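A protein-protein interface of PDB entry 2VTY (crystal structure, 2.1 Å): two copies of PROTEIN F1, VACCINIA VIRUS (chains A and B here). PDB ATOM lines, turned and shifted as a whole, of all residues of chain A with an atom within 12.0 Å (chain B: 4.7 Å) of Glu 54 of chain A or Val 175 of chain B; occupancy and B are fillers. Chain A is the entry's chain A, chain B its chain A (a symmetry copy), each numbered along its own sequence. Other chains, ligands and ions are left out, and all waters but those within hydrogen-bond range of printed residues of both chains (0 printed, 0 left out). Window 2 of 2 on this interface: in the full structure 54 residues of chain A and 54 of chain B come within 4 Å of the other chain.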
ATOM      1  N   ILE A  47      17.661  -8.676  38.553  1.00  0.00           N
ATOM      2  CA  ILE A  47      18.972  -8.874  37.911  1.00  0.00           C
ATOM      3  C   ILE A  47      19.040  -8.056  36.639  1.00  0.00           C
ATOM      4  O   ILE A  47      20.126  -7.677  36.216  1.00  0.00           O
ATOM      5  CB  ILE A  47      19.255 -10.348  37.348  1.00  0.00           C
ATOM      6  CG1 ILE A  47      18.057 -11.253  37.392  1.00  0.00           C
ATOM      7  CG2 ILE A  47      20.576 -10.992  37.763  1.00  0.00           C
ATOM      8  CD1 ILE A  47      17.241 -11.110  36.182  1.00  0.00           C
ATOM      9  N   LEU A  48      17.901  -7.809  35.990  1.00  0.00           N
ATOM     10  CA  LEU A  48      17.925  -7.131  34.695  1.00  0.00           C
ATOM     11  C   LEU A  48      18.446  -5.702  34.789  1.00  0.00           C
ATOM     12  O   LEU A  48      19.027  -5.211  33.843  1.00  0.00           O
ATOM     13  CB  LEU A  48      16.564  -7.187  33.981  1.00  0.00           C
ATOM     14  CG  LEU A  48      16.019  -8.590  33.687  1.00  0.00           C
ATOM     15  CD1 LEU A  48      14.577  -8.529  33.046  1.00  0.00           C
ATOM     16  CD2 LEU A  48      17.001  -9.384  32.830  1.00  0.00           C
ATOM     17  N   ASP A  49      18.238  -5.038  35.928  1.00  0.00           N
ATOM     18  CA  ASP A  49      18.847  -3.725  36.158  1.00  0.00           C
ATOM     19  C   ASP A  49      20.371  -3.794  36.192  1.00  0.00           C
ATOM     20  O   ASP A  49      21.023  -2.773  36.004  1.00  0.00           O
ATOM     21  CB  ASP A  49      18.393  -3.136  37.489  1.00  0.00           C
ATOM     22  CG  ASP A  49      16.897  -2.831  37.529  1.00  0.00           C
ATOM     23  OD1 ASP A  49      16.235  -2.705  36.465  1.00  0.00           O
ATOM     24  OD2 ASP A  49      16.392  -2.714  38.663  1.00  0.00           O
ATOM     25  N   TYR A  50      20.937  -4.979  36.437  1.00  0.00           N
ATOM     26  CA  TYR A  50      22.397  -5.191  36.428  1.00  0.00           C
ATOM     27  C   TYR A  50      22.924  -5.648  35.063  1.00  0.00           C
ATOM     28  O   TYR A  50      24.123  -5.793  34.863  1.00  0.00           O
ATOM     29  CB  TYR A  50      22.802  -6.180  37.555  1.00  0.00           C
ATOM     30  CG  TYR A  50      22.468  -5.596  38.916  1.00  0.00           C
ATOM     31  CD1 TYR A  50      21.149  -5.626  39.419  1.00  0.00           C
ATOM     32  CD2 TYR A  50      23.452  -4.945  39.671  1.00  0.00           C
ATOM     33  CE1 TYR A  50      20.837  -5.055  40.646  1.00  0.00           C
ATOM     34  CE2 TYR A  50      23.151  -4.365  40.893  1.00  0.00           C
ATOM     35  CZ  TYR A  50      21.854  -4.422  41.373  1.00  0.00           C
ATOM     36  OH  TYR A  50      21.592  -3.839  42.585  1.00  0.00           O
ATOM     37  N   LEU A  51      22.022  -5.890  34.125  1.00  0.00           N
ATOM     38  CA  LEU A  51      22.419  -6.379  32.836  1.00  0.00           C
ATOM     39  C   LEU A  51      22.028  -5.339  31.780  1.00  0.00           C
ATOM     40  O   LEU A  51      21.347  -5.690  30.821  1.00  0.00           O
ATOM     41  CB  LEU A  51      21.769  -7.770  32.569  1.00  0.00           C
ATOM     42  CG  LEU A  51      22.076  -8.958  33.517  1.00  0.00           C
ATOM     43  CD1 LEU A  51      21.130 -10.179  33.292  1.00  0.00           C
ATOM     44  CD2 LEU A  51      23.523  -9.388  33.341  1.00  0.00           C
ATOM     45  N   SER A  52      22.496  -4.089  31.929  1.00  0.00           N
ATOM     46  CA  SER A  52      22.004  -2.971  31.100  1.00  0.00           C
ATOM     47  C   SER A  52      22.610  -2.924  29.713  1.00  0.00           C
ATOM     48  O   SER A  52      21.970  -2.402  28.753  1.00  0.00           O
ATOM     49  CB  SER A  52      22.274  -1.618  31.762  1.00  0.00           C
ATOM     50  OG  SER A  52      21.923  -1.658  33.133  1.00  0.00           O
ATOM     51  N   THR A  53      23.837  -3.428  29.595  1.00  0.00           N
ATOM     52  CA  THR A  53      24.577  -3.354  28.326  1.00  0.00           C
ATOM     53  C   THR A  53      24.883  -4.803  27.925  1.00  0.00           C
ATOM     54  O   THR A  53      24.756  -5.696  28.743  1.00  0.00           O
ATOM     55  CB  THR A  53      25.906  -2.566  28.496  1.00  0.00           C
ATOM     56  OG1 THR A  53      26.761  -3.256  29.418  1.00  0.00           O
ATOM     57  CG2 THR A  53      25.684  -1.163  29.048  1.00  0.00           C
ATOM     58  N   GLU A  54      25.273  -5.022  26.682  1.00  0.00           N
ATOM     59  CA  GLU A  54      25.830  -6.298  26.213  1.00  0.00           C
ATOM     60  C   GLU A  54      27.050  -6.733  27.028  1.00  0.00           C
ATOM     61  O   GLU A  54      27.141  -7.889  27.418  1.00  0.00           O
ATOM     62  CB  GLU A  54      26.187  -6.221  24.712  1.00  0.00           C
ATOM     63  CG  GLU A  54      24.973  -6.130  23.786  1.00  0.00           C
ATOM     64  CD  GLU A  54      24.134  -7.425  23.813  1.00  0.00           C
ATOM     65  OE1 GLU A  54      23.043  -7.449  23.200  1.00  0.00           O
ATOM     66  OE2 GLU A  54      24.559  -8.417  24.447  1.00  0.00           O
ATOM     67  N   ARG A  55      27.980  -5.805  27.286  1.00  0.00           N
ATOM     68  CA  ARG A  55      29.112  -6.076  28.171  1.00  0.00           C
ATOM     69  C   ARG A  55      28.703  -6.621  29.524  1.00  0.00           C
ATOM     70  O   ARG A  55      29.293  -7.584  29.997  1.00  0.00           O
ATOM     71  CB  ARG A  55      30.102  -4.895  28.303  1.00  0.00           C
ATOM     72  CG  ARG A  55      31.338  -5.268  29.191  1.00  0.00           C
ATOM     73  CD  ARG A  55      32.388  -4.136  29.242  1.00  0.00           C
ATOM     74  NE  ARG A  55      33.688  -4.571  29.787  1.00  0.00           N
ATOM     75  CZ  ARG A  55      34.269  -4.008  30.841  1.00  0.00           C
ATOM     76  NH1 ARG A  55      35.423  -4.464  31.303  1.00  0.00           N
ATOM     77  NH2 ARG A  55      33.679  -2.985  31.442  1.00  0.00           N
ATOM     78  N   ASP A  56      27.674  -6.061  30.139  1.00  0.00           N
ATOM     79  CA  ASP A  56      27.188  -6.609  31.398  1.00  0.00           C
ATOM     80  C   ASP A  56      26.720  -8.059  31.267  1.00  0.00           C
ATOM     81  O   ASP A  56      26.981  -8.867  32.165  1.00  0.00           O
ATOM     82  CB  ASP A  56      26.024  -5.797  31.941  1.00  0.00           C
ATOM     83  CG  ASP A  56      26.436  -4.406  32.397  1.00  0.00           C
ATOM     84  OD1 ASP A  56      27.551  -4.201  32.922  1.00  0.00           O
ATOM     85  OD2 ASP A  56      25.595  -3.518  32.241  1.00  0.00           O
ATOM     86  N   HIS A  57      25.969  -8.365  30.201  1.00  0.00           N
ATOM     87  CA  HIS A  57      25.556  -9.750  29.932  1.00  0.00           C
ATOM     88  C   HIS A  57      26.733 -10.699  29.779  1.00  0.00           C
ATOM     89  O   HIS A  57      26.715 -11.778  30.340  1.00  0.00           O
ATOM     90  CB  HIS A  57      24.682  -9.857  28.669  1.00  0.00           C
ATOM     91  CG  HIS A  57      23.227  -9.606  28.924  1.00  0.00           C
ATOM     92  ND1 HIS A  57      22.637  -8.378  28.709  1.00  0.00           N
ATOM     93  CD2 HIS A  57      22.246 -10.420  29.374  1.00  0.00           C
ATOM     94  CE1 HIS A  57      21.350  -8.446  29.012  1.00  0.00           C
ATOM     95  NE2 HIS A  57      21.089  -9.677  29.413  1.00  0.00           N
ATOM     96  N   VAL A  58      27.729 -10.310  28.982  1.00  0.00           N
ATOM     97  CA  VAL A  58      28.893 -11.158  28.726  1.00  0.00           C
ATOM     98  C   VAL A  58      29.732 -11.383  30.004  1.00  0.00           C
ATOM     99  O   VAL A  58      30.220 -12.491  30.273  1.00  0.00           O
ATOM    100  CB  VAL A  58      29.786 -10.582  27.555  1.00  0.00           C
ATOM    101  CG1 VAL A  58      30.976 -11.500  27.285  1.00  0.00           C
ATOM    102  CG2 VAL A  58      28.950 -10.388  26.257  1.00  0.00           C
ATOM    103  N   MET A  59      29.890 -10.345  30.801  1.00  0.00           N
ATOM    104  CA  MET A  59      30.652 -10.460  32.056  1.00  0.00           C
ATOM    105  C   MET A  59      29.927 -11.364  33.011  1.00  0.00           C
ATOM    106  O   MET A  59      30.546 -12.177  33.655  1.00  0.00           O
ATOM    107  CB  MET A  59      30.826  -9.094  32.728  1.00  0.00           C
ATOM    108  CG  MET A  59      31.878  -8.237  32.083  1.00  0.00           C
ATOM    109  SD  MET A  59      32.383  -6.760  33.053  1.00  0.00           S
ATOM    110  CE  MET A  59      30.915  -5.733  33.138  1.00  0.00           C
ATOM    111  N   MET A  60      28.598 -11.236  33.087  1.00  0.00           N
ATOM    112  CA  MET A  60      27.814 -12.158  33.896  1.00  0.00           C
ATOM    113  C   MET A  60      28.009 -13.631  33.432  1.00  0.00           C
ATOM    114  O   MET A  60      28.122 -14.560  34.233  1.00  0.00           O
ATOM    115  CB  MET A  60      26.348 -11.757  33.805  1.00  0.00           C
ATOM    116  CG  MET A  60      25.360 -12.713  34.522  1.00  0.00           C
ATOM    117  SD  MET A  60      25.493 -12.652  36.316  1.00  0.00           S
ATOM    118  CE  MET A  60      24.683 -11.097  36.627  1.00  0.00           C
ATOM    119  N   ALA A  61      27.990 -13.841  32.129  1.00  0.00           N
ATOM    120  CA  ALA A  61      28.177 -15.170  31.571  1.00  0.00           C
ATOM    121  C   ALA A  61      29.554 -15.713  31.934  1.00  0.00           C
ATOM    122  O   ALA A  61      29.666 -16.879  32.324  1.00  0.00           O
ATOM    123  CB  ALA A  61      27.992 -15.144  30.020  1.00  0.00           C
ATOM    124  N   VAL A  62      30.593 -14.880  31.800  1.00  0.00           N
ATOM    125  CA  VAL A  62      31.954 -15.279  32.163  1.00  0.00           C
ATOM    126  C   VAL A  62      32.063 -15.659  33.656  1.00  0.00           C
ATOM    127  O   VAL A  62      32.528 -16.752  33.980  1.00  0.00           O
ATOM    128  CB  VAL A  62      33.031 -14.193  31.742  1.00  0.00           C
ATOM    129  CG1 VAL A  62      34.417 -14.534  32.318  1.00  0.00           C
ATOM    130  CG2 VAL A  62      33.074 -14.050  30.204  1.00  0.00           C
ATOM    131  N   ARG A  63      31.594 -14.778  34.537  1.00  0.00           N
ATOM    132  CA  ARG A  63      31.594 -15.045  35.980  1.00  0.00           C
ATOM    133  C   ARG A  63      30.777 -16.287  36.387  1.00  0.00           C
ATOM    134  O   ARG A  63      31.178 -17.045  37.272  1.00  0.00           O
ATOM    135  CB  ARG A  63      31.094 -13.822  36.757  1.00  0.00           C
ATOM    136  CG  ARG A  63      32.155 -13.164  37.662  1.00  0.00           C
ATOM    137  CD  ARG A  63      31.728 -11.765  38.140  1.00  0.00           C
ATOM    138  NE  ARG A  63      31.734 -10.786  37.035  1.00  0.00           N
ATOM    139  CZ  ARG A  63      31.490  -9.483  37.147  1.00  0.00           C
ATOM    140  NH1 ARG A  63      31.224  -8.912  38.321  1.00  0.00           N
ATOM    141  NH2 ARG A  63      31.510  -8.738  36.070  1.00  0.00           N
ATOM    142  N   LYS B  81      19.140 -14.417  26.599  1.00  0.00           N
ATOM    143  CA  LYS B  81      20.312 -13.742  26.074  1.00  0.00           C
ATOM    144  C   LYS B  81      21.562 -14.180  26.834  1.00  0.00           C
ATOM    145  O   LYS B  81      22.498 -14.642  26.225  1.00  0.00           O
ATOM    146  CB  LYS B  81      20.167 -12.226  26.115  1.00  0.00           C
ATOM    147  CG  LYS B  81      21.445 -11.490  25.684  1.00  0.00           C
ATOM    148  CD  LYS B  81      21.182  -9.988  25.535  1.00  0.00           C
ATOM    149  CE  LYS B  81      20.733  -9.697  24.125  1.00  0.00           C
ATOM    150  NZ  LYS B  81      20.491  -8.260  24.102  1.00  0.00           N
ATOM    151  N   TYR B  85      25.010 -16.758  25.888  1.00  0.00           N
ATOM    152  CA  TYR B  85      26.415 -16.333  26.076  1.00  0.00           C
ATOM    153  C   TYR B  85      27.169 -17.354  26.932  1.00  0.00           C
ATOM    154  O   TYR B  85      28.284 -17.727  26.599  1.00  0.00           O
ATOM    155  CB  TYR B  85      26.511 -14.913  26.684  1.00  0.00           C
ATOM    156  CG  TYR B  85      25.916 -13.808  25.818  1.00  0.00           C
ATOM    157  CD1 TYR B  85      25.770 -12.522  26.314  1.00  0.00           C
ATOM    158  CD2 TYR B  85      25.515 -14.048  24.484  1.00  0.00           C
ATOM    159  CE1 TYR B  85      25.242 -11.508  25.535  1.00  0.00           C
ATOM    160  CE2 TYR B  85      24.991 -13.002  23.674  1.00  0.00           C
ATOM    161  CZ  TYR B  85      24.860 -11.751  24.219  1.00  0.00           C
ATOM    162  OH  TYR B  85      24.318 -10.726  23.484  1.00  0.00           O
ATOM    163  N   CYS B 170      36.466  -9.356  29.291  1.00  0.00           N
ATOM    164  CA  CYS B 170      35.383  -8.788  28.492  1.00  0.00           C
ATOM    165  C   CYS B 170      35.742  -7.408  27.931  1.00  0.00           C
ATOM    166  O   CYS B 170      35.101  -6.406  28.258  1.00  0.00           O
ATOM    167  CB  CYS B 170      34.049  -8.796  29.234  1.00  0.00           C
ATOM    168  SG  CYS B 170      33.577 -10.492  29.795  1.00  0.00           S
ATOM    169  N   ASP B 171      36.763  -7.364  27.072  1.00  0.00           N
ATOM    170  CA  ASP B 171      37.040  -6.121  26.324  1.00  0.00           C
ATOM    171  C   ASP B 171      36.021  -5.976  25.196  1.00  0.00           C
ATOM    172  O   ASP B 171      35.171  -6.869  25.004  1.00  0.00           O
ATOM    173  CB  ASP B 171      38.505  -5.977  25.835  1.00  0.00           C
ATOM    174  CG  ASP B 171      38.985  -7.148  25.008  1.00  0.00           C
ATOM    175  OD1 ASP B 171      38.195  -8.074  24.722  1.00  0.00           O
ATOM    176  OD2 ASP B 171      40.187  -7.170  24.628  1.00  0.00           O
ATOM    177  N   ASP B 172      36.086  -4.853  24.465  1.00  0.00           N
ATOM    178  CA  ASP B 172      35.127  -4.586  23.404  1.00  0.00           C
ATOM    179  C   ASP B 172      35.254  -5.661  22.350  1.00  0.00           C
ATOM    180  O   ASP B 172      34.272  -6.065  21.748  1.00  0.00           O
ATOM    181  CB  ASP B 172      35.371  -3.201  22.793  1.00  0.00           C
ATOM    182  CG  ASP B 172      34.874  -2.052  23.700  1.00  0.00           C
ATOM    183  OD1 ASP B 172      34.086  -2.295  24.642  1.00  0.00           O
ATOM    184  OD2 ASP B 172      35.258  -0.890  23.455  1.00  0.00           O
ATOM    185  N   CYS B 173      36.477  -6.125  22.146  1.00  0.00           N
ATOM    186  CA  CYS B 173      36.768  -7.200  21.213  1.00  0.00           C
ATOM    187  C   CYS B 173      36.028  -8.513  21.580  1.00  0.00           C
ATOM    188  O   CYS B 173      35.325  -9.120  20.747  1.00  0.00           O
ATOM    189  CB  CYS B 173      38.308  -7.343  21.062  1.00  0.00           C
ATOM    190  SG  CYS B 173      38.894  -8.848  20.257  1.00  0.00           S
ATOM    191  N   PHE B 174      36.118  -8.923  22.836  1.00  0.00           N
ATOM    192  CA  PHE B 174      35.425 -10.130  23.263  1.00  0.00           C
ATOM    193  C   PHE B 174      33.894  -9.966  23.164  1.00  0.00           C
ATOM    194  O   PHE B 174      33.190 -10.846  22.677  1.00  0.00           O
ATOM    195  CB  PHE B 174      35.832 -10.491  24.705  1.00  0.00           C
ATOM    196  CG  PHE B 174      35.287 -11.812  25.190  1.00  0.00           C
ATOM    197  CD1 PHE B 174      35.641 -12.996  24.559  1.00  0.00           C
ATOM    198  CD2 PHE B 174      34.426 -11.864  26.296  1.00  0.00           C
ATOM    199  CE1 PHE B 174      35.153 -14.238  25.026  1.00  0.00           C
ATOM    200  CE2 PHE B 174      33.915 -13.117  26.775  1.00  0.00           C
ATOM    201  CZ  PHE B 174      34.289 -14.288  26.149  1.00  0.00           C
ATOM    202  N   VAL B 175      33.379  -8.840  23.634  1.00  0.00           N
ATOM    203  CA  VAL B 175      31.928  -8.588  23.578  1.00  0.00           C
ATOM    204  C   VAL B 175      31.425  -8.647  22.128  1.00  0.00           C
ATOM    205  O   VAL B 175      30.372  -9.228  21.847  1.00  0.00           O
ATOM    206  CB  VAL B 175      31.554  -7.244  24.241  1.00  0.00           C
ATOM    207  CG1 VAL B 175      30.028  -6.976  24.122  1.00  0.00           C
ATOM    208  CG2 VAL B 175      32.035  -7.223  25.707  1.00  0.00           C
ATOM    209  N   ASP B 176      32.175  -8.020  21.213  1.00  0.00           N
ATOM    210  CA  ASP B 176      31.856  -8.059  19.786  1.00  0.00           C
ATOM    211  C   ASP B 176      31.827  -9.480  19.223  1.00  0.00           C
ATOM    212  O   ASP B 176      30.930  -9.816  18.502  1.00  0.00           O
ATOM    213  CB  ASP B 176      32.862  -7.244  19.012  1.00  0.00           C
ATOM    214  CG  ASP B 176      32.637  -5.748  19.140  1.00  0.00           C
ATOM    215  OD1 ASP B 176      31.594  -5.284  19.671  1.00  0.00           O
ATOM    216  OD2 ASP B 176      33.542  -5.031  18.698  1.00  0.00           O
ATOM    217  N   TYR B 177      32.819 -10.304  19.529  1.00  0.00           N
ATOM    218  CA  TYR B 177      32.787 -11.725  19.142  1.00  0.00           C
ATOM    219  C   TYR B 177      31.543 -12.458  19.641  1.00  0.00           C
ATOM    220  O   TYR B 177      30.851 -13.134  18.864  1.00  0.00           O
ATOM    221  CB  TYR B 177      34.004 -12.456  19.701  1.00  0.00           C
ATOM    222  CG  TYR B 177      35.262 -12.259  18.899  1.00  0.00           C
ATOM    223  CD1 TYR B 177      35.316 -12.638  17.553  1.00  0.00           C
ATOM    224  CD2 TYR B 177      36.408 -11.727  19.487  1.00  0.00           C
ATOM    225  CE1 TYR B 177      36.490 -12.495  16.808  1.00  0.00           C
ATOM    226  CE2 TYR B 177      37.580 -11.580  18.764  1.00  0.00           C
ATOM    227  CZ  TYR B 177      37.615 -11.961  17.430  1.00  0.00           C
ATOM    228  OH  TYR B 177      38.770 -11.801  16.710  1.00  0.00           O
ATOM    229  N   ILE B 178      31.298 -12.346  20.945  1.00  0.00           N
ATOM    230  CA  ILE B 178      30.206 -13.047  21.610  1.00  0.00           C
ATOM    231  C   ILE B 178      28.806 -12.633  21.090  1.00  0.00           C
ATOM    232  O   ILE B 178      27.977 -13.492  20.751  1.00  0.00           O
ATOM    233  CB  ILE B 178      30.278 -12.861  23.141  1.00  0.00           C
ATOM    234  CG1 ILE B 178      31.539 -13.544  23.722  1.00  0.00           C
ATOM    235  CG2 ILE B 178      29.001 -13.422  23.798  1.00  0.00           C
ATOM    236  CD1 ILE B 178      31.626 -15.056  23.494  1.00  0.00           C
ATOM    237  N   THR B 179      28.535 -11.333  20.999  1.00  0.00           N
ATOM    238  CA  THR B 179      27.299 -10.905  20.338  1.00  0.00           C
ATOM    239  C   THR B 179      27.204 -11.293  18.854  1.00  0.00           C
ATOM    240  O   THR B 179      26.135 -11.556  18.384  1.00  0.00           O
ATOM    241  CB  THR B 179      27.006  -9.391  20.518  1.00  0.00           C
ATOM    242  OG1 THR B 179      27.993  -8.629  19.836  1.00  0.00           O
ATOM    243  CG2 THR B 179      27.012  -9.036  21.983  1.00  0.00           C
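NZ of Lys 81 of chain B is in salt-bridge range of OE1 of Glu 54 of chain A.
OE2 of Glu 54 of chain A lies within hydrogen-bond range of OH of Tyr 85 of chain B (2.5 Å).
The guanidinium group (NE) of Arg 55 of chain A sits at hydrogen-bond distance from the backbone carbonyl oxygen (O) of Cys 170 of chain B, at 2.8 Å.
The backbone carbonyl oxygen of Thr 53 of chain A is in hydrogen-bond range of a ring nitrogen (ND1) of His 57 of chain A, 3.4 Å away.
The guanidinium group of Arg 63 of chain A lies close to the side-chain sulfur of Met 59 of chain A, at 3.7 Å.
The side-chain carboxylate (OD1) of Asp 171 of chain B sits at hydrogen-bond distance from the backbone NH (N) of Phe 174 of chain B, at 2.9 Å.
The backbone carbonyl oxygen of Val 175 of chain B is in hydrogen-bond range of the side-chain hydroxyl of Thr 179 of chain B.
The backbone carbonyl oxygen (O) of Asp 176 of chain B lies within hydrogen-bond range of the side-chain hydroxyl (OG1) of Thr 179 of chain B (3.4 Å).
Among the printed residues, merely in contact across the chains: Glu 54 of chain A with Val 175 of chain B, Glu 54 of chain A with Thr 179 of chain B, Arg 55 of chain A with Val 175 of chain B, His 57 of chain A with Lys 81 of chain B, His 57 of chain A with Tyr 85 of chain B, Val 58 of chain A with Tyr 85 of chain B, Val 58 of chain A with Cys 170 of chain B, Val 58 of chain A with Phe 174 of chain B, Val 58 of chain A with Ile 178 of chain B, Met 59 of chain A with Cys 170 of chain B, Ala 61 of chain A with Tyr 85 of chain B, Val 62 of chain A with Cys 170 of chain B and Val 62 of chain A with Phe 174 of chain B.
Of chain B, only Lys 81 (2.8 Å), Tyr 85 (2.5 Å), Val 175 (3.96 Å) and Thr 179 (3.5 Å) come within 4 Å of Glu 54 of chain A.
Val 175 of chain B touches just these residues of chain A: Glu 54 (3.96 Å) and Arg 55 (3.9 Å).
No residue of chain A comes within 4 Å of Asp 171 of chain B.
No residue of chain A comes within 4 Å of Asp 172 of chain B.
Phe 174 of chain B touches just these residues of chain A: Val 58 and Val 62.
Of the printed residues of chain A, Ile 178 of chain B touches Val 58 (3.9 Å).
Of the printed residues of chain B, His 57 of chain A touches Lys 81 and Tyr 85.
Of the printed residues of chain B, Val 62 of chain A touches Cys 170 and Phe 174.
Printed residues of chain B within 4 Å of Met 59 of chain A: Cys 170.
Of the printed residues of chain B, Arg 55 of chain A touches Cys 170 and Val 175.
Of the printed residues of chain B, Ala 61 of chain A touches Tyr 85.
Ser 52 of chain A touches none of the printed residues of chain B.
Hydrophobic or aromatic side chains of chain B within 4 Å of the printed part of chain A: Tyr 85, Phe 174, Val 175 and Ile 178.
Of the 17 printed residues of chain A, 7 touch a printed residue of chain B.
Hydrophobic or aromatic side chains of chain A that line the printed part of chain B: His 57, Val 58, Met 59, Ala 61 and Val 62.
Along chain A the printed residues that touch a printed residue of chain B span positions 54 to 62.
Among the printed residues, 16 pairs touch across the chains.
No position is printed for both chains.
Of the 16 pairs that touch across the chains among the printed residues, none has its exchanged pair printed and touching as well.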
